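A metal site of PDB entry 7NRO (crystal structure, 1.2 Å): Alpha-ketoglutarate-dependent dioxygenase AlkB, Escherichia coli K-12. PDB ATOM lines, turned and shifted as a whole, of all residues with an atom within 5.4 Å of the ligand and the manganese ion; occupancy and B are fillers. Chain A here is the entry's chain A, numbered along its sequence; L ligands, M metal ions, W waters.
OH of Tyr 122 lies within hydrogen-bond range of O6 of the ligand, at 2.8 Å. O2 of the ligand sits at hydrogen-bond distance from ND2 of Asn 120 (2.8 Å). NH1 of Arg 204 lies within salt-bridge range of O6 of the ligand, 2.8 Å away. An oxygen (O3) of the ligand sits at hydrogen-bond distance from the side-chain hydroxyl (OH) of Tyr 76, 3.2 Å away. O1 of the ligand lies close to OD1 of Asn 206 (3.3 Å).
OH of Tyr 122 lies within hydrogen-bond range of ND2 of Asn 120 (3.2 Å). The backbone NH (N) of Tyr 122 sits at hydrogen-bond distance from the backbone carbonyl oxygen (O) of Arg 204 (2.8 Å). OD1 of Asn 206 lies within hydrogen-bond range of NH2 of Arg 204, at 3.2 Å. NH2 of Arg 204 lies within hydrogen-bond range of OG of Ser 147. The side-chain hydroxyl of Ser 147 sits at hydrogen-bond distance from the side-chain amide oxygen of Asn 206, 3.4 Å away. O of Leu 118 is in hydrogen-bond range of N of Thr 208, 2.9 Å away. The backbone NH (N) of Leu 128 is in hydrogen-bond range of the backbone carbonyl oxygen (O) of Ile 189. The guanidinium group (NH2) of Arg 210 sits at hydrogen-bond distance from the side-chain hydroxyl (OG1) of Thr 208.
Merely in contact with the ligand: Leu 118, Leu 128, Ile 189, Trp 69, Met 61, Arg 210, Gln 132, Phe 154 and Leu 170. 17 residues have an atom within 4 Å of the ligand: Met 61, Trp 69, Tyr 76, Leu 118, Asn 120, Tyr 122, Leu 128, His 131, Gln 132, Asp 133, Phe 154, Leu 170, His 187, Ile 189, Arg 204, Asn 206 and Arg 210.
Three residues have an atom within 4 Å of the manganese ion: His 131, Asp 133 and His 187. The nearest printed residue that does not touch the manganese ion is Arg 210 (4.5 Å).
OD1 of Asp 133 is bound to the manganese ion, 2.1 Å away. The manganese ion is bound by O5 of the ligand, 2.2 Å away. The manganese ion is bound by NE2 of His 187, 2.2 Å away. NE2 of His 131 binds the manganese ion (2.2 Å). N1 of the ligand is bound to the manganese ion, at 2.2 Å. Water W3 is bound to the manganese ion, 2.4 Å away. The manganese ion has six donor atoms within binding distance.
Water W3 bridges NH2 of Arg 210 (3.4 Å) and OD2 of Asp 133 (3.4 Å). Water W2 lies within hydrogen-bond range of O2 of the ligand (2.7 Å), OG1 of Thr 208 (2.7 Å), O of Asn 206 (2.9 Å) and O of Leu 118 (3.3 Å). Water W5 lies within hydrogen-bond range of OG of Ser 145 (2.5 Å) and O1 of the ligand (2.8 Å). Water W4 bridges O of Gln 132 and O4 of the ligand.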
ATOM      1  N   THR A  51     -19.684   8.779 -33.077  1.00  0.00           N
ATOM      2  CA  THR A  51     -19.973   8.794 -31.666  1.00  0.00           C
ATOM      3  C   THR A  51     -21.474   8.913 -31.442  1.00  0.00           C
ATOM      4  O   THR A  51     -22.242   9.205 -32.361  1.00  0.00           O
ATOM      5  CB  THR A  51     -19.321   9.994 -30.986  1.00  0.00           C
ATOM      6  OG1 THR A  51     -19.973  11.192 -31.459  1.00  0.00           O
ATOM      7  CG2 THR A  51     -17.882  10.084 -31.306  1.00  0.00           C
ATOM      8  N   MET A  57     -15.345  10.058 -35.511  1.00  0.00           N
ATOM      9  CA  MET A  57     -14.080  10.113 -34.809  1.00  0.00           C
ATOM     10  C   MET A  57     -12.944  10.275 -35.800  1.00  0.00           C
ATOM     11  O   MET A  57     -12.968   9.762 -36.916  1.00  0.00           O
ATOM     12  CB  MET A  57     -13.905   8.826 -34.017  1.00  0.00           C
ATOM     13  CG  MET A  57     -14.931   8.645 -32.936  1.00  0.00           C
ATOM     14  SD  MET A  57     -14.734   7.074 -32.083  1.00  0.00           S
ATOM     15  CE  MET A  57     -13.486   7.456 -30.894  1.00  0.00           C
ATOM     16  N   MET A  61     -10.643   2.556 -36.198  1.00  0.00           N
ATOM     17  CA  MET A  61     -10.516   1.415 -35.314  1.00  0.00           C
ATOM     18  C   MET A  61     -10.969   0.125 -35.977  1.00  0.00           C
ATOM     19  O   MET A  61     -11.710   0.124 -36.956  1.00  0.00           O
ATOM     20  CB  MET A  61     -11.352   1.644 -34.060  1.00  0.00           C
ATOM     21  CG  MET A  61     -10.889   2.818 -33.229  1.00  0.00           C
ATOM     22  SD  MET A  61     -11.783   2.865 -31.644  1.00  0.00           S
ATOM     23  CE  MET A  61     -11.553   4.587 -31.213  1.00  0.00           C
ATOM     24  N   TRP A  69     -15.096  -3.798 -29.495  1.00  0.00           N
ATOM     25  CA  TRP A  69     -15.736  -2.563 -29.066  1.00  0.00           C
ATOM     26  C   TRP A  69     -16.228  -1.802 -30.278  1.00  0.00           C
ATOM     27  O   TRP A  69     -15.494  -1.622 -31.243  1.00  0.00           O
ATOM     28  CB  TRP A  69     -14.706  -1.758 -28.296  1.00  0.00           C
ATOM     29  CG  TRP A  69     -15.203  -0.550 -27.636  1.00  0.00           C
ATOM     30  CD1 TRP A  69     -15.737  -0.485 -26.374  1.00  0.00           C
ATOM     31  CD2 TRP A  69     -15.188   0.777 -28.155  1.00  0.00           C
ATOM     32  NE1 TRP A  69     -16.062   0.829 -26.069  1.00  0.00           N
ATOM     33  CE2 TRP A  69     -15.700   1.625 -27.130  1.00  0.00           C
ATOM     34  CE3 TRP A  69     -14.777   1.350 -29.347  1.00  0.00           C
ATOM     35  CZ2 TRP A  69     -15.838   3.008 -27.292  1.00  0.00           C
ATOM     36  CZ3 TRP A  69     -14.899   2.745 -29.498  1.00  0.00           C
ATOM     37  CH2 TRP A  69     -15.420   3.543 -28.471  1.00  0.00           C
ATOM     38  N   TYR A  76     -22.206   2.590 -27.165  1.00  0.00           N
ATOM     39  CA  TYR A  76     -20.978   1.807 -27.254  1.00  0.00           C
ATOM     40  C   TYR A  76     -21.224   0.465 -26.580  1.00  0.00           C
ATOM     41  O   TYR A  76     -21.905   0.395 -25.553  1.00  0.00           O
ATOM     42  CB  TYR A  76     -19.823   2.500 -26.547  1.00  0.00           C
ATOM     43  CG  TYR A  76     -19.403   3.794 -27.193  1.00  0.00           C
ATOM     44  CD1 TYR A  76     -18.915   3.815 -28.491  1.00  0.00           C
ATOM     45  CD2 TYR A  76     -19.469   5.012 -26.503  1.00  0.00           C
ATOM     46  CE1 TYR A  76     -18.530   4.992 -29.107  1.00  0.00           C
ATOM     47  CE2 TYR A  76     -19.061   6.202 -27.103  1.00  0.00           C
ATOM     48  CZ  TYR A  76     -18.589   6.172 -28.405  1.00  0.00           C
ATOM     49  OH  TYR A  76     -18.200   7.336 -29.042  1.00  0.00           O
ATOM     50  N   LEU A 118      -8.994  -3.831 -29.015  1.00  0.00           N
ATOM     51  CA  LEU A 118      -9.333  -2.726 -29.881  1.00  0.00           C
ATOM     52  C   LEU A 118      -8.043  -2.179 -30.467  1.00  0.00           C
ATOM     53  O   LEU A 118      -7.076  -1.876 -29.743  1.00  0.00           O
ATOM     54  CB  LEU A 118     -10.019  -1.671 -29.037  1.00  0.00           C
ATOM     55  CG  LEU A 118     -10.564  -0.466 -29.798  1.00  0.00           C
ATOM     56  CD1 LEU A 118     -11.533  -0.715 -30.891  1.00  0.00           C
ATOM     57  CD2 LEU A 118     -11.230   0.485 -28.768  1.00  0.00           C
ATOM     58  N   ASN A 120      -6.480   0.816 -32.625  1.00  0.00           N
ATOM     59  CA  ASN A 120      -6.770   2.210 -32.921  1.00  0.00           C
ATOM     60  C   ASN A 120      -5.634   2.806 -33.726  1.00  0.00           C
ATOM     61  O   ASN A 120      -4.511   2.877 -33.253  1.00  0.00           O
ATOM     62  CB  ASN A 120      -6.968   2.932 -31.578  1.00  0.00           C
ATOM     63  CG  ASN A 120      -7.362   4.377 -31.745  1.00  0.00           C
ATOM     64  OD1 ASN A 120      -7.299   4.915 -32.858  1.00  0.00           O
ATOM     65  ND2 ASN A 120      -7.679   5.052 -30.653  1.00  0.00           N
ATOM     66  N   TYR A 122      -4.117   6.137 -35.474  1.00  0.00           N
ATOM     67  CA  TYR A 122      -4.068   7.605 -35.464  1.00  0.00           C
ATOM     68  C   TYR A 122      -3.278   8.051 -36.671  1.00  0.00           C
ATOM     69  O   TYR A 122      -2.087   7.790 -36.783  1.00  0.00           O
ATOM     70  CB  TYR A 122      -3.358   8.101 -34.217  1.00  0.00           C
ATOM     71  CG  TYR A 122      -4.010   7.839 -32.920  1.00  0.00           C
ATOM     72  CD1 TYR A 122      -3.979   6.555 -32.319  1.00  0.00           C
ATOM     73  CD2 TYR A 122      -4.674   8.851 -32.231  1.00  0.00           C
ATOM     74  CE1 TYR A 122      -4.573   6.316 -31.068  1.00  0.00           C
ATOM     75  CE2 TYR A 122      -5.249   8.617 -31.005  1.00  0.00           C
ATOM     76  CZ  TYR A 122      -5.213   7.369 -30.432  1.00  0.00           C
ATOM     77  OH  TYR A 122      -5.844   7.177 -29.205  1.00  0.00           O
ATOM     78  N   LEU A 128      -8.030  11.610 -29.386  1.00  0.00           N
ATOM     79  CA  LEU A 128      -9.115  11.007 -28.630  1.00  0.00           C
ATOM     80  C   LEU A 128      -9.418  11.924 -27.475  1.00  0.00           C
ATOM     81  O   LEU A 128      -8.543  12.127 -26.616  1.00  0.00           O
ATOM     82  CB  LEU A 128      -8.660   9.685 -28.049  1.00  0.00           C
ATOM     83  CG  LEU A 128      -9.232   8.397 -28.639  1.00  0.00           C
ATOM     84  CD1 LEU A 128      -8.861   7.263 -27.629  1.00  0.00           C
ATOM     85  CD2 LEU A 128     -10.706   8.439 -28.983  1.00  0.00           C
ATOM     86  N   HIS A 131     -11.951  10.853 -21.836  1.00  0.00           N
ATOM     87  CA  HIS A 131     -13.021   9.893 -21.627  1.00  0.00           C
ATOM     88  C   HIS A 131     -12.574   8.909 -20.555  1.00  0.00           C
ATOM     89  O   HIS A 131     -11.413   8.812 -20.191  1.00  0.00           O
ATOM     90  CB  HIS A 131     -13.364   9.116 -22.900  1.00  0.00           C
ATOM     91  CG  HIS A 131     -12.234   8.256 -23.362  1.00  0.00           C
ATOM     92  ND1 HIS A 131     -11.160   8.755 -24.072  1.00  0.00           N
ATOM     93  CD2 HIS A 131     -11.962   6.965 -23.122  1.00  0.00           C
ATOM     94  CE1 HIS A 131     -10.299   7.777 -24.265  1.00  0.00           C
ATOM     95  NE2 HIS A 131     -10.768   6.682 -23.715  1.00  0.00           N
ATOM     96  N   GLN A 132     -13.536   8.110 -20.081  1.00  0.00           N
ATOM     97  CA  GLN A 132     -13.292   6.915 -19.276  1.00  0.00           C
ATOM     98  C   GLN A 132     -13.660   5.684 -20.074  1.00  0.00           C
ATOM     99  O   GLN A 132     -14.553   5.717 -20.909  1.00  0.00           O
ATOM    100  CB  GLN A 132     -14.116   6.955 -17.995  1.00  0.00           C
ATOM    101  CG  GLN A 132     -13.691   7.986 -16.979  1.00  0.00           C
ATOM    102  CD  GLN A 132     -14.612   7.995 -15.782  1.00  0.00           C
ATOM    103  OE1 GLN A 132     -14.187   7.738 -14.651  1.00  0.00           O
ATOM    104  NE2 GLN A 132     -15.882   8.242 -16.024  1.00  0.00           N
ATOM    105  N   ASP A 133     -13.013   4.561 -19.771  1.00  0.00           N
ATOM    106  CA  ASP A 133     -13.406   3.261 -20.296  1.00  0.00           C
ATOM    107  C   ASP A 133     -14.150   2.557 -19.179  1.00  0.00           C
ATOM    108  O   ASP A 133     -13.542   2.028 -18.233  1.00  0.00           O
ATOM    109  CB  ASP A 133     -12.158   2.481 -20.691  1.00  0.00           C
ATOM    110  CG  ASP A 133     -11.610   2.883 -22.003  1.00  0.00           C
ATOM    111  OD1 ASP A 133     -10.948   3.909 -22.070  1.00  0.00           O
ATOM    112  OD2 ASP A 133     -11.889   2.207 -23.012  1.00  0.00           O
ATOM    113  N   ASP A 135     -17.095   0.500 -20.049  1.00  0.00           N
ATOM    114  CA  ASP A 135     -18.037  -0.393 -20.724  1.00  0.00           C
ATOM    115  C   ASP A 135     -17.796  -1.864 -20.403  1.00  0.00           C
ATOM    116  O   ASP A 135     -18.562  -2.717 -20.868  1.00  0.00           O
ATOM    117  CB  ASP A 135     -17.914  -0.211 -22.245  1.00  0.00           C
ATOM    118  CG  ASP A 135     -18.309   1.170 -22.698  1.00  0.00           C
ATOM    119  OD1 ASP A 135     -19.407   1.627 -22.288  1.00  0.00           O
ATOM    120  OD2 ASP A 135     -17.529   1.797 -23.455  1.00  0.00           O
ATOM    121  N   SER A 145      -2.365  -1.510 -22.730  1.00  0.00           N
ATOM    122  CA  SER A 145      -2.327  -0.568 -23.850  1.00  0.00           C
ATOM    123  C   SER A 145      -0.942  -0.504 -24.477  1.00  0.00           C
ATOM    124  O   SER A 145      -0.014  -0.039 -23.822  1.00  0.00           O
ATOM    125  CB  SER A 145      -2.623   0.848 -23.334  1.00  0.00           C
ATOM    126  OG  SER A 145      -2.193   1.774 -24.336  1.00  0.00           O
ATOM    127  N   SER A 147       1.553   0.836 -27.549  1.00  0.00           N
ATOM    128  CA  SER A 147       1.781   1.878 -28.536  1.00  0.00           C
ATOM    129  C   SER A 147       2.765   1.435 -29.589  1.00  0.00           C
ATOM    130  O   SER A 147       3.801   0.839 -29.257  1.00  0.00           O
ATOM    131  CB  SER A 147       2.405   3.089 -27.854  1.00  0.00           C
ATOM    132  OG  SER A 147       1.520   3.766 -26.978  1.00  0.00           O
ATOM    133  N   PHE A 154      -0.202  11.321 -24.230  1.00  0.00           N
ATOM    134  CA  PHE A 154      -1.307  10.789 -23.475  1.00  0.00           C
ATOM    135  C   PHE A 154      -1.567  11.655 -22.253  1.00  0.00           C
ATOM    136  O   PHE A 154      -0.650  11.986 -21.483  1.00  0.00           O
ATOM    137  CB  PHE A 154      -0.906   9.396 -23.027  1.00  0.00           C
ATOM    138  CG  PHE A 154      -1.987   8.653 -22.258  1.00  0.00           C
ATOM    139  CD1 PHE A 154      -2.927   7.898 -22.889  1.00  0.00           C
ATOM    140  CD2 PHE A 154      -2.038   8.709 -20.898  1.00  0.00           C
ATOM    141  CE1 PHE A 154      -3.900   7.186 -22.182  1.00  0.00           C
ATOM    142  CE2 PHE A 154      -3.011   7.986 -20.189  1.00  0.00           C
ATOM    143  CZ  PHE A 154      -3.941   7.247 -20.852  1.00  0.00           C
ATOM    144  N   LEU A 170       3.972   8.683 -25.093  1.00  0.00           N
ATOM    145  CA  LEU A 170       4.003   7.261 -25.329  1.00  0.00           C
ATOM    146  C   LEU A 170       4.643   7.031 -26.673  1.00  0.00           C
ATOM    147  O   LEU A 170       4.206   7.619 -27.687  1.00  0.00           O
ATOM    148  CB  LEU A 170       2.612   6.669 -25.314  1.00  0.00           C
ATOM    149  CG  LEU A 170       1.888   6.776 -23.991  1.00  0.00           C
ATOM    150  CD1 LEU A 170       0.493   6.200 -24.072  1.00  0.00           C
ATOM    151  CD2 LEU A 170       2.670   6.110 -22.873  1.00  0.00           C
ATOM    152  N   HIS A 187      -8.933  10.029 -19.488  1.00  0.00           N
ATOM    153  CA  HIS A 187      -7.701  10.062 -20.256  1.00  0.00           C
ATOM    154  C   HIS A 187      -8.036  10.351 -21.706  1.00  0.00           C
ATOM    155  O   HIS A 187      -9.193  10.222 -22.158  1.00  0.00           O
ATOM    156  CB  HIS A 187      -6.913   8.745 -20.093  1.00  0.00           C
ATOM    157  CG  HIS A 187      -7.702   7.558 -20.563  1.00  0.00           C
ATOM    158  ND1 HIS A 187      -8.650   6.936 -19.786  1.00  0.00           N
ATOM    159  CD2 HIS A 187      -7.710   6.893 -21.744  1.00  0.00           C
ATOM    160  CE1 HIS A 187      -9.250   5.983 -20.502  1.00  0.00           C
ATOM    161  NE2 HIS A 187      -8.656   5.900 -21.676  1.00  0.00           N
ATOM    162  N   ILE A 189      -5.783  11.319 -25.845  1.00  0.00           N
ATOM    163  CA  ILE A 189      -4.582  11.448 -26.652  1.00  0.00           C
ATOM    164  C   ILE A 189      -4.712  12.748 -27.422  1.00  0.00           C
ATOM    165  O   ILE A 189      -5.741  12.992 -28.077  1.00  0.00           O
ATOM    166  CB  ILE A 189      -4.435  10.258 -27.615  1.00  0.00           C
ATOM    167  CG1 ILE A 189      -4.055   8.986 -26.845  1.00  0.00           C
ATOM    168  CG2 ILE A 189      -3.420  10.589 -28.703  1.00  0.00           C
ATOM    169  CD1 ILE A 189      -2.598   8.923 -26.575  1.00  0.00           C
ATOM    170  N   ARG A 204       0.313   6.152 -35.906  1.00  0.00           N
ATOM    171  CA  ARG A 204       0.449   5.451 -34.650  1.00  0.00           C
ATOM    172  C   ARG A 204      -0.653   4.422 -34.570  1.00  0.00           C
ATOM    173  O   ARG A 204      -1.805   4.698 -34.954  1.00  0.00           O
ATOM    174  CB  ARG A 204       0.305   6.418 -33.494  1.00  0.00           C
ATOM    175  CG  ARG A 204       0.289   5.763 -32.146  1.00  0.00           C
ATOM    176  CD  ARG A 204       0.183   6.811 -31.051  1.00  0.00           C
ATOM    177  NE  ARG A 204       0.244   6.259 -29.685  1.00  0.00           N
ATOM    178  CZ  ARG A 204      -0.792   6.101 -28.859  1.00  0.00           C
ATOM    179  NH1 ARG A 204      -2.016   6.481 -29.163  1.00  0.00           N
ATOM    180  NH2 ARG A 204      -0.572   5.584 -27.656  1.00  0.00           N
ATOM    181  N   ASN A 206      -2.507   2.024 -31.491  1.00  0.00           N
ATOM    182  CA  ASN A 206      -2.552   1.640 -30.094  1.00  0.00           C
ATOM    183  C   ASN A 206      -3.480   0.446 -29.954  1.00  0.00           C
ATOM    184  O   ASN A 206      -4.636   0.475 -30.431  1.00  0.00           O
ATOM    185  CB  ASN A 206      -3.100   2.756 -29.241  1.00  0.00           C
ATOM    186  CG  ASN A 206      -2.853   2.503 -27.764  1.00  0.00           C
ATOM    187  OD1 ASN A 206      -1.722   2.655 -27.297  1.00  0.00           O
ATOM    188  ND2 ASN A 206      -3.846   2.094 -27.057  1.00  0.00           N
ATOM    189  N   THR A 208      -5.566  -1.829 -27.283  1.00  0.00           N
ATOM    190  CA  THR A 208      -6.047  -1.899 -25.906  1.00  0.00           C
ATOM    191  C   THR A 208      -6.759  -3.229 -25.715  1.00  0.00           C
ATOM    192  O   THR A 208      -7.823  -3.510 -26.301  1.00  0.00           O
ATOM    193  CB  THR A 208      -6.962  -0.746 -25.502  1.00  0.00           C
ATOM    194  OG1 THR A 208      -7.917  -0.404 -26.498  1.00  0.00           O
ATOM    195  CG2 THR A 208      -6.155   0.487 -25.128  1.00  0.00           C
ATOM    196  N   ARG A 210      -8.774  -5.884 -23.479  1.00  0.00           N
ATOM    197  CA  ARG A 210      -9.848  -5.757 -22.510  1.00  0.00           C
ATOM    198  C   ARG A 210     -10.464  -7.115 -22.227  1.00  0.00           C
ATOM    199  O   ARG A 210     -10.570  -7.978 -23.121  1.00  0.00           O
ATOM    200  CB  ARG A 210     -10.962  -4.863 -23.079  1.00  0.00           C
ATOM    201  CG  ARG A 210     -10.499  -3.447 -23.518  1.00  0.00           C
ATOM    202  CD  ARG A 210     -10.906  -3.013 -24.944  1.00  0.00           C
ATOM    203  NE  ARG A 210     -10.399  -1.675 -25.298  1.00  0.00           N
ATOM    204  CZ  ARG A 210     -10.784  -0.547 -24.691  1.00  0.00           C
ATOM    205  NH1 ARG A 210     -11.873  -0.504 -23.938  1.00  0.00           N
ATOM    206  NH2 ARG A 210     -10.048   0.570 -24.816  1.00  0.00           N
HETATM  207  N1  LIG L   1      -9.831   4.198 -25.492  1.00  0.00           N
HETATM  208  C1  LIG L   1     -15.298   5.684 -24.564  1.00  0.00           C
HETATM  209  C2  LIG L   1     -15.271   6.657 -25.544  1.00  0.00           C
HETATM  210  N2  LIG L   1     -12.061   4.186 -25.371  1.00  0.00           N
HETATM  211  C3  LIG L   1     -14.238   6.764 -26.441  1.00  0.00           C
HETATM  212  O1  LIG L   1      -2.865   5.491 -25.943  1.00  0.00           O
HETATM  213  C4  LIG L   1      -5.096   4.987 -25.539  1.00  0.00           C
HETATM  214  O2  LIG L   1      -7.452   3.650 -28.215  1.00  0.00           O
HETATM  215  C5  LIG L   1     -13.224   4.837 -25.415  1.00  0.00           C
HETATM  216  C6  LIG L   1     -14.261   4.773 -24.502  1.00  0.00           C
HETATM  217  N3  LIG L   1     -16.415   7.570 -25.665  1.00  0.00           N
HETATM  218  C7  LIG L   1     -10.971   3.969 -26.134  1.00  0.00           C
HETATM  219  O3  LIG L   1     -16.410   8.395 -26.561  1.00  0.00           O
HETATM  220  C8  LIG L   1      -8.673   4.140 -26.201  1.00  0.00           C
HETATM  221  O4  LIG L   1     -17.348   7.435 -24.877  1.00  0.00           O
HETATM  222  C9  LIG L   1      -3.969   5.369 -26.483  1.00  0.00           C
HETATM  223  N4  LIG L   1      -6.338   4.581 -26.155  1.00  0.00           N
HETATM  224  C10 LIG L   1      -7.494   4.613 -25.479  1.00  0.00           C
HETATM  225  O5  LIG L   1      -7.617   5.013 -24.320  1.00  0.00           O
HETATM  226  C11 LIG L   1     -13.209   5.833 -26.382  1.00  0.00           C
HETATM  227  C12 LIG L   1     -11.026   3.613 -27.479  1.00  0.00           C
HETATM  228  C13 LIG L   1      -9.839   3.478 -28.165  1.00  0.00           C
HETATM  229  C14 LIG L   1      -8.628   3.754 -27.540  1.00  0.00           C
HETATM  230  O6  LIG L   1      -4.235   5.492 -27.686  1.00  0.00           O
HETATM  231 MN    MN M   1      -9.556   4.824 -23.352  1.00  0.00          MN
HETATM  232  O   HOH W   1      -5.829   3.667 -22.291  1.00  0.00           O
HETATM  233  O   HOH W   2      -6.701   1.113 -28.425  1.00  0.00           O
HETATM  234  O   HOH W   3      -8.540   2.734 -22.733  1.00  0.00           O
HETATM  235  O   HOH W   4     -17.025   6.628 -21.855  1.00  0.00           O
HETATM  236  O   HOH W   5      -2.226   4.107 -23.567  1.00  0.00           O
